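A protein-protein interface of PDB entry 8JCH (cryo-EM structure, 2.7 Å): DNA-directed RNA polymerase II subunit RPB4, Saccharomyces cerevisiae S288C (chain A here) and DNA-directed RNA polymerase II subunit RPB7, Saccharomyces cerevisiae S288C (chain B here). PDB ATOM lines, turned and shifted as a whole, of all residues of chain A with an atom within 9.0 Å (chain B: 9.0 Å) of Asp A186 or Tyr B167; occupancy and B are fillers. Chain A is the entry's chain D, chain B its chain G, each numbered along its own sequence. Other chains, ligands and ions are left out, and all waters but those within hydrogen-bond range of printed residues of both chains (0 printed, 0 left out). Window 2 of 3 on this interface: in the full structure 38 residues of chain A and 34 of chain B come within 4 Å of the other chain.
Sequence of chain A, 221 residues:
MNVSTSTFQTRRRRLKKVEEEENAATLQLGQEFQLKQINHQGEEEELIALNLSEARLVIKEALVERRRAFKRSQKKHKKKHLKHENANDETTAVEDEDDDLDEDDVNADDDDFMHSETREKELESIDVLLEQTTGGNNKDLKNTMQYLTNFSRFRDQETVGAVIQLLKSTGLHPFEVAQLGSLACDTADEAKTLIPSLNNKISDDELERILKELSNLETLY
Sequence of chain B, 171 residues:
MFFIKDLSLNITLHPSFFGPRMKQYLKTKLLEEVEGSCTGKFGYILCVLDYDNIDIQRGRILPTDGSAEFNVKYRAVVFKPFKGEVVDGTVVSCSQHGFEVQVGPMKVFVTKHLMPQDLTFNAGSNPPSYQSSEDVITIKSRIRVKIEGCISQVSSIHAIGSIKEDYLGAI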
ATOM      1  N   ARG A 153     -22.241 -34.960   8.582  1.00  0.00           N
ATOM      2  CA  ARG A 153     -20.871 -34.896   8.086  1.00  0.00           C
ATOM      3  C   ARG A 153     -20.028 -36.090   8.509  1.00  0.00           C
ATOM      4  O   ARG A 153     -19.244 -36.602   7.706  1.00  0.00           O
ATOM      5  CB  ARG A 153     -20.198 -33.605   8.560  1.00  0.00           C
ATOM      6  CG  ARG A 153     -18.963 -33.220   7.763  1.00  0.00           C
ATOM      7  CD  ARG A 153     -18.472 -31.835   8.147  1.00  0.00           C
ATOM      8  NE  ARG A 153     -17.227 -31.487   7.471  1.00  0.00           N
ATOM      9  CZ  ARG A 153     -16.610 -30.320   7.594  1.00  0.00           C
ATOM     10  NH1 ARG A 153     -17.093 -29.358   8.363  1.00  0.00           N
ATOM     11  NH2 ARG A 153     -15.477 -30.113   6.928  1.00  0.00           N
ATOM     12  N   LEU A 180     -17.581 -24.524  12.745  1.00  0.00           N
ATOM     13  CA  LEU A 180     -16.591 -24.966  11.768  1.00  0.00           C
ATOM     14  C   LEU A 180     -16.611 -26.480  11.592  1.00  0.00           C
ATOM     15  O   LEU A 180     -16.329 -26.975  10.496  1.00  0.00           O
ATOM     16  CB  LEU A 180     -15.191 -24.481  12.156  1.00  0.00           C
ATOM     17  CG  LEU A 180     -14.554 -24.918  13.475  1.00  0.00           C
ATOM     18  CD1 LEU A 180     -13.686 -26.153  13.287  1.00  0.00           C
ATOM     19  CD2 LEU A 180     -13.735 -23.776  14.054  1.00  0.00           C
ATOM     20  N   LEU A 183     -20.249 -26.857   9.395  1.00  0.00           N
ATOM     21  CA  LEU A 183     -20.165 -26.272   8.064  1.00  0.00           C
ATOM     22  C   LEU A 183     -18.890 -26.716   7.357  1.00  0.00           C
ATOM     23  O   LEU A 183     -17.830 -26.853   7.975  1.00  0.00           O
ATOM     24  CB  LEU A 183     -20.211 -24.745   8.147  1.00  0.00           C
ATOM     25  CG  LEU A 183     -21.581 -24.073   8.296  1.00  0.00           C
ATOM     26  CD1 LEU A 183     -22.536 -24.559   7.214  1.00  0.00           C
ATOM     27  CD2 LEU A 183     -22.174 -24.289   9.682  1.00  0.00           C
ATOM     28  N   ALA A 184     -18.998 -26.942   6.051  1.00  0.00           N
ATOM     29  CA  ALA A 184     -17.853 -27.344   5.253  1.00  0.00           C
ATOM     30  C   ALA A 184     -16.947 -26.148   4.976  1.00  0.00           C
ATOM     31  O   ALA A 184     -17.332 -24.988   5.143  1.00  0.00           O
ATOM     32  CB  ALA A 184     -18.308 -27.977   3.938  1.00  0.00           C
ATOM     33  N   CYS A 185     -15.723 -26.447   4.546  1.00  0.00           N
ATOM     34  CA  CYS A 185     -14.743 -25.408   4.267  1.00  0.00           C
ATOM     35  C   CYS A 185     -13.710 -25.946   3.289  1.00  0.00           C
ATOM     36  O   CYS A 185     -13.584 -27.157   3.094  1.00  0.00           O
ATOM     37  CB  CYS A 185     -14.063 -24.918   5.549  1.00  0.00           C
ATOM     38  SG  CYS A 185     -12.718 -25.983   6.117  1.00  0.00           S
ATOM     39  N   ASP A 186     -12.974 -25.024   2.678  1.00  0.00           N
ATOM     40  CA  ASP A 186     -11.881 -25.358   1.773  1.00  0.00           C
ATOM     41  C   ASP A 186     -10.552 -24.745   2.182  1.00  0.00           C
ATOM     42  O   ASP A 186      -9.509 -25.383   2.014  1.00  0.00           O
ATOM     43  CB  ASP A 186     -12.231 -24.933   0.335  1.00  0.00           C
ATOM     44  CG  ASP A 186     -12.661 -23.478   0.235  1.00  0.00           C
ATOM     45  OD1 ASP A 186     -13.526 -23.181  -0.614  1.00  0.00           O
ATOM     46  OD2 ASP A 186     -12.153 -22.635   1.001  1.00  0.00           O
ATOM     47  N   THR A 187     -10.558 -23.527   2.713  1.00  0.00           N
ATOM     48  CA  THR A 187      -9.348 -22.896   3.231  1.00  0.00           C
ATOM     49  C   THR A 187      -9.762 -21.869   4.281  1.00  0.00           C
ATOM     50  O   THR A 187     -10.913 -21.846   4.731  1.00  0.00           O
ATOM     51  CB  THR A 187      -8.519 -22.266   2.107  1.00  0.00           C
ATOM     52  OG1 THR A 187      -7.363 -21.628   2.667  1.00  0.00           O
ATOM     53  CG2 THR A 187      -9.336 -21.235   1.353  1.00  0.00           C
ATOM     54  N   ALA A 188      -8.816 -21.011   4.669  1.00  0.00           N
ATOM     55  CA  ALA A 188      -9.068 -20.072   5.756  1.00  0.00           C
ATOM     56  C   ALA A 188     -10.086 -19.006   5.374  1.00  0.00           C
ATOM     57  O   ALA A 188     -10.791 -18.488   6.248  1.00  0.00           O
ATOM     58  CB  ALA A 188      -7.758 -19.416   6.194  1.00  0.00           C
ATOM     59  N   ASP A 189     -10.175 -18.658   4.087  1.00  0.00           N
ATOM     60  CA  ASP A 189     -11.076 -17.584   3.679  1.00  0.00           C
ATOM     61  C   ASP A 189     -12.532 -17.949   3.945  1.00  0.00           C
ATOM     62  O   ASP A 189     -13.315 -17.106   4.399  1.00  0.00           O
ATOM     63  CB  ASP A 189     -10.821 -17.217   2.207  1.00  0.00           C
ATOM     64  CG  ASP A 189     -11.492 -18.164   1.205  1.00  0.00           C
ATOM     65  OD1 ASP A 189     -10.785 -18.613   0.278  1.00  0.00           O
ATOM     66  OD2 ASP A 189     -12.712 -18.420   1.281  1.00  0.00           O
ATOM     67  N   GLU A 190     -12.914 -19.199   3.672  1.00  0.00           N
ATOM     68  CA  GLU A 190     -14.291 -19.619   3.919  1.00  0.00           C
ATOM     69  C   GLU A 190     -14.627 -19.560   5.404  1.00  0.00           C
ATOM     70  O   GLU A 190     -15.702 -19.084   5.784  1.00  0.00           O
ATOM     71  CB  GLU A 190     -14.519 -21.028   3.374  1.00  0.00           C
ATOM     72  CG  GLU A 190     -15.974 -21.473   3.410  1.00  0.00           C
ATOM     73  CD  GLU A 190     -16.236 -22.691   2.548  1.00  0.00           C
ATOM     74  OE1 GLU A 190     -15.291 -23.159   1.877  1.00  0.00           O
ATOM     75  OE2 GLU A 190     -17.384 -23.182   2.542  1.00  0.00           O
ATOM     76  N   ALA A 191     -13.714 -20.030   6.258  1.00  0.00           N
ATOM     77  CA  ALA A 191     -13.959 -19.990   7.695  1.00  0.00           C
ATOM     78  C   ALA A 191     -14.051 -18.555   8.200  1.00  0.00           C
ATOM     79  O   ALA A 191     -14.900 -18.239   9.041  1.00  0.00           O
ATOM     80  CB  ALA A 191     -12.860 -20.751   8.437  1.00  0.00           C
ATOM     81  N   LYS A 192     -13.178 -17.675   7.702  1.00  0.00           N
ATOM     82  CA  LYS A 192     -13.209 -16.281   8.134  1.00  0.00           C
ATOM     83  C   LYS A 192     -14.487 -15.584   7.682  1.00  0.00           C
ATOM     84  O   LYS A 192     -15.077 -14.807   8.442  1.00  0.00           O
ATOM     85  CB  LYS A 192     -11.978 -15.543   7.608  1.00  0.00           C
ATOM     86  CG  LYS A 192     -10.675 -15.968   8.264  1.00  0.00           C
ATOM     87  CD  LYS A 192     -10.701 -15.714   9.762  1.00  0.00           C
ATOM     88  CE  LYS A 192     -10.281 -14.290  10.088  1.00  0.00           C
ATOM     89  NZ  LYS A 192      -8.862 -14.033   9.713  1.00  0.00           N
ATOM     90  N   THR A 193     -14.928 -15.843   6.450  1.00  0.00           N
ATOM     91  CA  THR A 193     -16.112 -15.172   5.925  1.00  0.00           C
ATOM     92  C   THR A 193     -17.406 -15.744   6.489  1.00  0.00           C
ATOM     93  O   THR A 193     -18.414 -15.031   6.548  1.00  0.00           O
ATOM     94  CB  THR A 193     -16.132 -15.254   4.397  1.00  0.00           C
ATOM     95  OG1 THR A 193     -15.609 -16.520   3.977  1.00  0.00           O
ATOM     96  CG2 THR A 193     -15.293 -14.139   3.791  1.00  0.00           C
ATOM     97  N   LEU A 194     -17.404 -17.016   6.897  1.00  0.00           N
ATOM     98  CA  LEU A 194     -18.640 -17.655   7.343  1.00  0.00           C
ATOM     99  C   LEU A 194     -19.186 -16.991   8.602  1.00  0.00           C
ATOM    100  O   LEU A 194     -20.389 -16.723   8.702  1.00  0.00           O
ATOM    101  CB  LEU A 194     -18.404 -19.148   7.579  1.00  0.00           C
ATOM    102  CG  LEU A 194     -18.725 -20.081   6.407  1.00  0.00           C
ATOM    103  CD1 LEU A 194     -18.813 -21.525   6.879  1.00  0.00           C
ATOM    104  CD2 LEU A 194     -20.011 -19.663   5.709  1.00  0.00           C
ATOM    105  N   ILE A 195     -18.322 -16.712   9.571  1.00  0.00           N
ATOM    106  CA  ILE A 195     -18.766 -16.088  10.816  1.00  0.00           C
ATOM    107  C   ILE A 195     -17.879 -14.891  11.154  1.00  0.00           C
ATOM    108  O   ILE A 195     -16.696 -14.868  10.783  1.00  0.00           O
ATOM    109  CB  ILE A 195     -18.868 -17.139  11.947  1.00  0.00           C
ATOM    110  CG1 ILE A 195     -17.532 -17.812  12.336  1.00  0.00           C
ATOM    111  CG2 ILE A 195     -19.915 -18.202  11.608  1.00  0.00           C
ATOM    112  CD1 ILE A 195     -16.449 -16.966  12.969  1.00  0.00           C
ATOM    113  N   LEU A 207      -4.989 -22.225  11.956  1.00  0.00           N
ATOM    114  CA  LEU A 207      -6.326 -22.301  11.379  1.00  0.00           C
ATOM    115  C   LEU A 207      -6.335 -23.166  10.126  1.00  0.00           C
ATOM    116  O   LEU A 207      -7.154 -24.081   9.996  1.00  0.00           O
ATOM    117  CB  LEU A 207      -6.845 -20.896  11.068  1.00  0.00           C
ATOM    118  CG  LEU A 207      -8.147 -20.816  10.267  1.00  0.00           C
ATOM    119  CD1 LEU A 207      -9.301 -21.419  11.056  1.00  0.00           C
ATOM    120  CD2 LEU A 207      -8.453 -19.378   9.879  1.00  0.00           C
ATOM    121  N   GLU A 208      -5.420 -22.904   9.192  1.00  0.00           N
ATOM    122  CA  GLU A 208      -5.366 -23.738   7.997  1.00  0.00           C
ATOM    123  C   GLU A 208      -4.978 -25.171   8.341  1.00  0.00           C
ATOM    124  O   GLU A 208      -5.484 -26.111   7.716  1.00  0.00           O
ATOM    125  CB  GLU A 208      -4.405 -23.140   6.966  1.00  0.00           C
ATOM    126  CG  GLU A 208      -2.941 -23.135   7.367  1.00  0.00           C
ATOM    127  CD  GLU A 208      -2.171 -24.298   6.772  1.00  0.00           C
ATOM    128  OE1 GLU A 208      -2.322 -24.557   5.561  1.00  0.00           O
ATOM    129  OE2 GLU A 208      -1.414 -24.954   7.519  1.00  0.00           O
ATOM    130  N   LEU A 211      -7.996 -26.852   9.763  1.00  0.00           N
ATOM    131  CA  LEU A 211      -8.998 -26.911   8.706  1.00  0.00           C
ATOM    132  C   LEU A 211      -8.715 -28.057   7.744  1.00  0.00           C
ATOM    133  O   LEU A 211      -9.632 -28.792   7.363  1.00  0.00           O
ATOM    134  CB  LEU A 211      -9.060 -25.578   7.959  1.00  0.00           C
ATOM    135  CG  LEU A 211      -9.958 -24.500   8.572  1.00  0.00           C
ATOM    136  CD1 LEU A 211     -10.378 -23.486   7.520  1.00  0.00           C
ATOM    137  CD2 LEU A 211     -11.177 -25.113   9.250  1.00  0.00           C
ATOM    138  N   LYS A 212      -7.451 -28.241   7.350  1.00  0.00           N
ATOM    139  CA  LYS A 212      -7.107 -29.401   6.529  1.00  0.00           C
ATOM    140  C   LYS A 212      -7.285 -30.698   7.310  1.00  0.00           C
ATOM    141  O   LYS A 212      -7.680 -31.726   6.740  1.00  0.00           O
ATOM    142  CB  LYS A 212      -5.676 -29.290   5.998  1.00  0.00           C
ATOM    143  CG  LYS A 212      -5.298 -27.979   5.298  1.00  0.00           C
ATOM    144  CD  LYS A 212      -6.332 -27.510   4.276  1.00  0.00           C
ATOM    145  CE  LYS A 212      -7.189 -26.362   4.805  1.00  0.00           C
ATOM    146  NZ  LYS A 212      -8.377 -26.118   3.947  1.00  0.00           N
ATOM    147  N   GLU A 213      -6.992 -30.671   8.614  1.00  0.00           N
ATOM    148  CA  GLU A 213      -7.221 -31.850   9.441  1.00  0.00           C
ATOM    149  C   GLU A 213      -8.692 -32.251   9.424  1.00  0.00           C
ATOM    150  O   GLU A 213      -9.028 -33.422   9.209  1.00  0.00           O
ATOM    151  CB  GLU A 213      -6.745 -31.591  10.870  1.00  0.00           C
ATOM    152  CG  GLU A 213      -6.639 -32.847  11.721  1.00  0.00           C
ATOM    153  CD  GLU A 213      -5.997 -34.002  10.979  1.00  0.00           C
ATOM    154  OE1 GLU A 213      -4.757 -34.003  10.836  1.00  0.00           O
ATOM    155  OE2 GLU A 213      -6.733 -34.912  10.541  1.00  0.00           O
ATOM    156  N   LEU A 214      -9.587 -31.280   9.621  1.00  0.00           N
ATOM    157  CA  LEU A 214     -11.016 -31.558   9.560  1.00  0.00           C
ATOM    158  C   LEU A 214     -11.452 -31.953   8.154  1.00  0.00           C
ATOM    159  O   LEU A 214     -12.364 -32.771   7.999  1.00  0.00           O
ATOM    160  CB  LEU A 214     -11.809 -30.343  10.039  1.00  0.00           C
ATOM    161  CG  LEU A 214     -13.278 -30.591  10.383  1.00  0.00           C
ATOM    162  CD1 LEU A 214     -13.401 -31.418  11.653  1.00  0.00           C
ATOM    163  CD2 LEU A 214     -14.019 -29.273  10.522  1.00  0.00           C
ATOM    164  N   SER A 215     -10.816 -31.391   7.125  1.00  0.00           N
ATOM    165  CA  SER A 215     -11.155 -31.758   5.754  1.00  0.00           C
ATOM    166  C   SER A 215     -10.878 -33.234   5.500  1.00  0.00           C
ATOM    167  O   SER A 215     -11.724 -33.951   4.952  1.00  0.00           O
ATOM    168  CB  SER A 215     -10.377 -30.884   4.770  1.00  0.00           C
ATOM    169  OG  SER A 215     -10.775 -29.527   4.868  1.00  0.00           O
ATOM    170  N   GLU A 218     -13.271 -35.450   7.484  1.00  0.00           N
ATOM    171  CA  GLU A 218     -14.611 -35.535   6.922  1.00  0.00           C
ATOM    172  C   GLU A 218     -14.643 -36.217   5.563  1.00  0.00           C
ATOM    173  O   GLU A 218     -15.701 -36.717   5.166  1.00  0.00           O
ATOM    174  CB  GLU A 218     -15.236 -34.137   6.804  1.00  0.00           C
ATOM    175  CG  GLU A 218     -14.703 -33.292   5.659  1.00  0.00           C
ATOM    176  CD  GLU A 218     -15.649 -33.250   4.474  1.00  0.00           C
ATOM    177  OE1 GLU A 218     -16.790 -33.742   4.603  1.00  0.00           O
ATOM    178  OE2 GLU A 218     -15.251 -32.726   3.412  1.00  0.00           O
ATOM    179  N   VAL B  86     -24.815 -18.813  10.095  1.00  0.00           N
ATOM    180  CA  VAL B  86     -24.875 -19.440   8.780  1.00  0.00           C
ATOM    181  C   VAL B  86     -25.308 -20.890   8.952  1.00  0.00           C
ATOM    182  O   VAL B  86     -24.679 -21.651   9.695  1.00  0.00           O
ATOM    183  CB  VAL B  86     -23.522 -19.349   8.060  1.00  0.00           C
ATOM    184  CG1 VAL B  86     -23.482 -20.308   6.883  1.00  0.00           C
ATOM    185  CG2 VAL B  86     -23.262 -17.923   7.601  1.00  0.00           C
ATOM    186  N   ARG B 144     -27.089 -22.785   1.387  1.00  0.00           N
ATOM    187  CA  ARG B 144     -26.620 -22.227   2.647  1.00  0.00           C
ATOM    188  C   ARG B 144     -27.183 -20.822   2.799  1.00  0.00           C
ATOM    189  O   ARG B 144     -27.018 -19.984   1.906  1.00  0.00           O
ATOM    190  CB  ARG B 144     -25.092 -22.203   2.702  1.00  0.00           C
ATOM    191  CG  ARG B 144     -24.512 -22.475   4.078  1.00  0.00           C
ATOM    192  CD  ARG B 144     -22.997 -22.582   4.025  1.00  0.00           C
ATOM    193  NE  ARG B 144     -22.559 -23.898   3.575  1.00  0.00           N
ATOM    194  CZ  ARG B 144     -21.321 -24.185   3.194  1.00  0.00           C
ATOM    195  NH1 ARG B 144     -20.368 -23.268   3.195  1.00  0.00           N
ATOM    196  NH2 ARG B 144     -21.034 -25.423   2.802  1.00  0.00           N
ATOM    197  N   VAL B 145     -27.843 -20.567   3.926  1.00  0.00           N
ATOM    198  CA  VAL B 145     -28.575 -19.326   4.143  1.00  0.00           C
ATOM    199  C   VAL B 145     -28.251 -18.789   5.531  1.00  0.00           C
ATOM    200  O   VAL B 145     -28.199 -19.548   6.505  1.00  0.00           O
ATOM    201  CB  VAL B 145     -30.095 -19.540   3.972  1.00  0.00           C
ATOM    202  CG1 VAL B 145     -30.561 -20.751   4.768  1.00  0.00           C
ATOM    203  CG2 VAL B 145     -30.865 -18.299   4.378  1.00  0.00           C
ATOM    204  N   LYS B 146     -28.019 -17.482   5.614  1.00  0.00           N
ATOM    205  CA  LYS B 146     -27.782 -16.810   6.882  1.00  0.00           C
ATOM    206  C   LYS B 146     -29.102 -16.355   7.498  1.00  0.00           C
ATOM    207  O   LYS B 146     -30.137 -16.284   6.831  1.00  0.00           O
ATOM    208  CB  LYS B 146     -26.849 -15.613   6.688  1.00  0.00           C
ATOM    209  CG  LYS B 146     -25.977 -15.298   7.892  1.00  0.00           C
ATOM    210  CD  LYS B 146     -25.332 -13.927   7.761  1.00  0.00           C
ATOM    211  CE  LYS B 146     -24.251 -13.722   8.809  1.00  0.00           C
ATOM    212  NZ  LYS B 146     -23.077 -14.608   8.577  1.00  0.00           N
ATOM    213  N   ILE B 163     -29.207 -14.309   1.089  1.00  0.00           N
ATOM    214  CA  ILE B 163     -28.140 -14.938   0.317  1.00  0.00           C
ATOM    215  C   ILE B 163     -27.061 -13.951  -0.107  1.00  0.00           C
ATOM    216  O   ILE B 163     -25.988 -14.385  -0.554  1.00  0.00           O
ATOM    217  CB  ILE B 163     -28.696 -15.675  -0.923  1.00  0.00           C
ATOM    218  CG1 ILE B 163     -30.040 -16.340  -0.618  1.00  0.00           C
ATOM    219  CG2 ILE B 163     -27.724 -16.744  -1.403  1.00  0.00           C
ATOM    220  CD1 ILE B 163     -29.991 -17.372   0.495  1.00  0.00           C
ATOM    221  N   LYS B 164     -27.289 -12.645   0.036  1.00  0.00           N
ATOM    222  CA  LYS B 164     -26.339 -11.634  -0.429  1.00  0.00           C
ATOM    223  C   LYS B 164     -25.136 -11.611   0.509  1.00  0.00           C
ATOM    224  O   LYS B 164     -25.033 -10.800   1.434  1.00  0.00           O
ATOM    225  CB  LYS B 164     -27.006 -10.266  -0.515  1.00  0.00           C
ATOM    226  CG  LYS B 164     -26.128  -9.185  -1.129  1.00  0.00           C
ATOM    227  CD  LYS B 164     -26.844  -8.454  -2.254  1.00  0.00           C
ATOM    228  CE  LYS B 164     -28.074  -7.723  -1.745  1.00  0.00           C
ATOM    229  NZ  LYS B 164     -27.750  -6.813  -0.611  1.00  0.00           N
ATOM    230  N   GLU B 165     -24.207 -12.530   0.259  1.00  0.00           N
ATOM    231  CA  GLU B 165     -22.976 -12.623   1.031  1.00  0.00           C
ATOM    232  C   GLU B 165     -21.980 -13.463   0.244  1.00  0.00           C
ATOM    233  O   GLU B 165     -22.362 -14.442  -0.400  1.00  0.00           O
ATOM    234  CB  GLU B 165     -23.225 -13.238   2.414  1.00  0.00           C
ATOM    235  CG  GLU B 165     -21.980 -13.372   3.277  1.00  0.00           C
ATOM    236  CD  GLU B 165     -21.157 -12.098   3.314  1.00  0.00           C
ATOM    237  OE1 GLU B 165     -21.627 -11.101   3.902  1.00  0.00           O
ATOM    238  OE2 GLU B 165     -20.041 -12.094   2.755  1.00  0.00           O
ATOM    239  N   ASP B 166     -20.711 -13.065   0.295  1.00  0.00           N
ATOM    240  CA  ASP B 166     -19.671 -13.801  -0.411  1.00  0.00           C
ATOM    241  C   ASP B 166     -19.534 -15.211   0.151  1.00  0.00           C
ATOM    242  O   ASP B 166     -19.519 -15.414   1.368  1.00  0.00           O
ATOM    243  CB  ASP B 166     -18.336 -13.062  -0.308  1.00  0.00           C
ATOM    244  CG  ASP B 166     -17.174 -13.885  -0.827  1.00  0.00           C
ATOM    245  OD1 ASP B 166     -17.283 -14.436  -1.941  1.00  0.00           O
ATOM    246  OD2 ASP B 166     -16.150 -13.983  -0.117  1.00  0.00           O
ATOM    247  N   TYR B 167     -19.431 -16.187  -0.755  1.00  0.00           N
ATOM    248  CA  TYR B 167     -19.276 -17.597  -0.393  1.00  0.00           C
ATOM    249  C   TYR B 167     -20.398 -18.067   0.530  1.00  0.00           C
ATOM    250  O   TYR B 167     -20.160 -18.750   1.529  1.00  0.00           O
ATOM    251  CB  TYR B 167     -17.906 -17.857   0.239  1.00  0.00           C
ATOM    252  CG  TYR B 167     -17.322 -19.208  -0.108  1.00  0.00           C
ATOM    253  CD1 TYR B 167     -18.108 -20.201  -0.679  1.00  0.00           C
ATOM    254  CD2 TYR B 167     -15.984 -19.489   0.135  1.00  0.00           C
ATOM    255  CE1 TYR B 167     -17.579 -21.435  -0.997  1.00  0.00           C
ATOM    256  CE2 TYR B 167     -15.446 -20.721  -0.181  1.00  0.00           C
ATOM    257  CZ  TYR B 167     -16.248 -21.691  -0.746  1.00  0.00           C
ATOM    258  OH  TYR B 167     -15.719 -22.921  -1.063  1.00  0.00           O
ATOM    259  N   LEU B 168     -21.630 -17.700   0.195  1.00  0.00           N
ATOM    260  CA  LEU B 168     -22.797 -18.109   0.966  1.00  0.00           C
ATOM    261  C   LEU B 168     -23.807 -18.902   0.154  1.00  0.00           C
ATOM    262  O   LEU B 168     -24.392 -19.856   0.672  1.00  0.00           O
ATOM    263  CB  LEU B 168     -23.490 -16.881   1.574  1.00  0.00           C
ATOM    264  CG  LEU B 168     -24.561 -17.188   2.623  1.00  0.00           C
ATOM    265  CD1 LEU B 168     -23.921 -17.547   3.954  1.00  0.00           C
ATOM    266  CD2 LEU B 168     -25.523 -16.021   2.781  1.00  0.00           C
ATOM    267  N   GLY B 169     -24.030 -18.536  -1.106  1.00  0.00           N
ATOM    268  CA  GLY B 169     -25.003 -19.203  -1.943  1.00  0.00           C
ATOM    269  C   GLY B 169     -24.428 -20.414  -2.652  1.00  0.00           C
ATOM    270  O   GLY B 169     -23.344 -20.909  -2.337  1.00  0.00           O
ATOM    271  N   ALA B 170     -25.193 -20.900  -3.632  1.00  0.00           N
ATOM    272  CA  ALA B 170     -24.809 -22.034  -4.467  1.00  0.00           C
ATOM    273  C   ALA B 170     -24.536 -23.283  -3.636  1.00  0.00           C
ATOM    274  O   ALA B 170     -25.474 -23.925  -3.155  1.00  0.00           O
ATOM    275  CB  ALA B 170     -23.586 -21.685  -5.320  1.00  0.00           C
ATOM    276  N   ILE B 171     -23.254 -23.609  -3.460  1.00  0.00           N
ATOM    277  CA  ILE B 171     -22.757 -24.818  -2.781  1.00  0.00           C
ATOM    278  C   ILE B 171     -23.619 -26.069  -2.981  1.00  0.00           C
ATOM    279  O   ILE B 171     -24.319 -26.223  -3.983  1.00  0.00           O
ATOM    280  CB  ILE B 171     -22.508 -24.539  -1.254  1.00  0.00           C
ATOM    281  CG1 ILE B 171     -23.720 -23.932  -0.524  1.00  0.00           C
ATOM    282  CG2 ILE B 171     -21.283 -23.652  -1.070  1.00  0.00           C
ATOM    283  CD1 ILE B 171     -24.880 -24.874  -0.244  1.00  0.00           C
ATOM    284  OXT ILE B 171     -23.607 -26.984  -2.158  1.00  0.00           O
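The side-chain carboxylate of Asp A186 lies close to the side-chain hydroxyl of Tyr B167, at 2.3 Å.
OE2 of Glu A190 lies within salt-bridge range of NH1 of Arg B144, 3.1 Å away.
The side-chain carboxylate (OE1) of Glu A190 lies within hydrogen-bond range of the side-chain hydroxyl (OH) of Tyr B167, at 3.0 Å.
The side-chain amino group (NZ) of Lys B146 lies within hydrogen-bond range of the backbone carbonyl oxygen (O) of Leu A194.
The side-chain hydroxyl (OG1) of Thr A193 sits at hydrogen-bond distance from the backbone carbonyl oxygen (O) of Asp A189, 2.4 Å away.
The backbone carbonyl oxygen (O) of Glu A190 lies within hydrogen-bond range of the side-chain hydroxyl (OG1) of Thr A193 (3.1 Å).
The guanidinium group (NH1) of Arg A153 is in hydrogen-bond range of the backbone carbonyl oxygen (O) of Leu A183, 2.6 Å away.
The backbone NH (N) of Asp A186 lies within hydrogen-bond range of the side-chain carboxylate (OE1) of Glu A190 (3.1 Å).
No residue of chain B comes within 4 Å of Cys A185.
Asp A186 touches one residue of chain B.
Printed residues of chain B within 4 Å of Asp A189: Tyr B167.
Of the printed residues of chain B, Glu A190 touches Arg B144 and Tyr B167.
Leu A211 touches none of the printed residues of chain B.
Glu A218 touches none of the printed residues of chain B.
Printed residues of chain A within 4 Å of Val B86: Leu A183 (3.6 Å) and Leu A194 (3.3 Å).
Tyr B167 touches three residues of chain A.
The nearest residue of chain A that does not touch Tyr B167 is Leu A194 (4.3 Å).
The nearest printed residue of chain B that does not touch Leu A194 is Tyr B167 (4.3 Å).
Among the printed residues, pairs that only touch across the chains: Leu A183 with Val B86 (3.6 Å), Leu A183 with Arg B144 (3.7 Å), Ala A184 with Arg B144 (3.9 Å), Asp A189 with Tyr B167 (3.6 Å) and Leu A194 with Val B86 (3.3 Å).
Hydrophobic or aromatic side chains of chain A within 4 Å of the printed part of chain B: Leu A183, Ala A184 and Leu A194.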
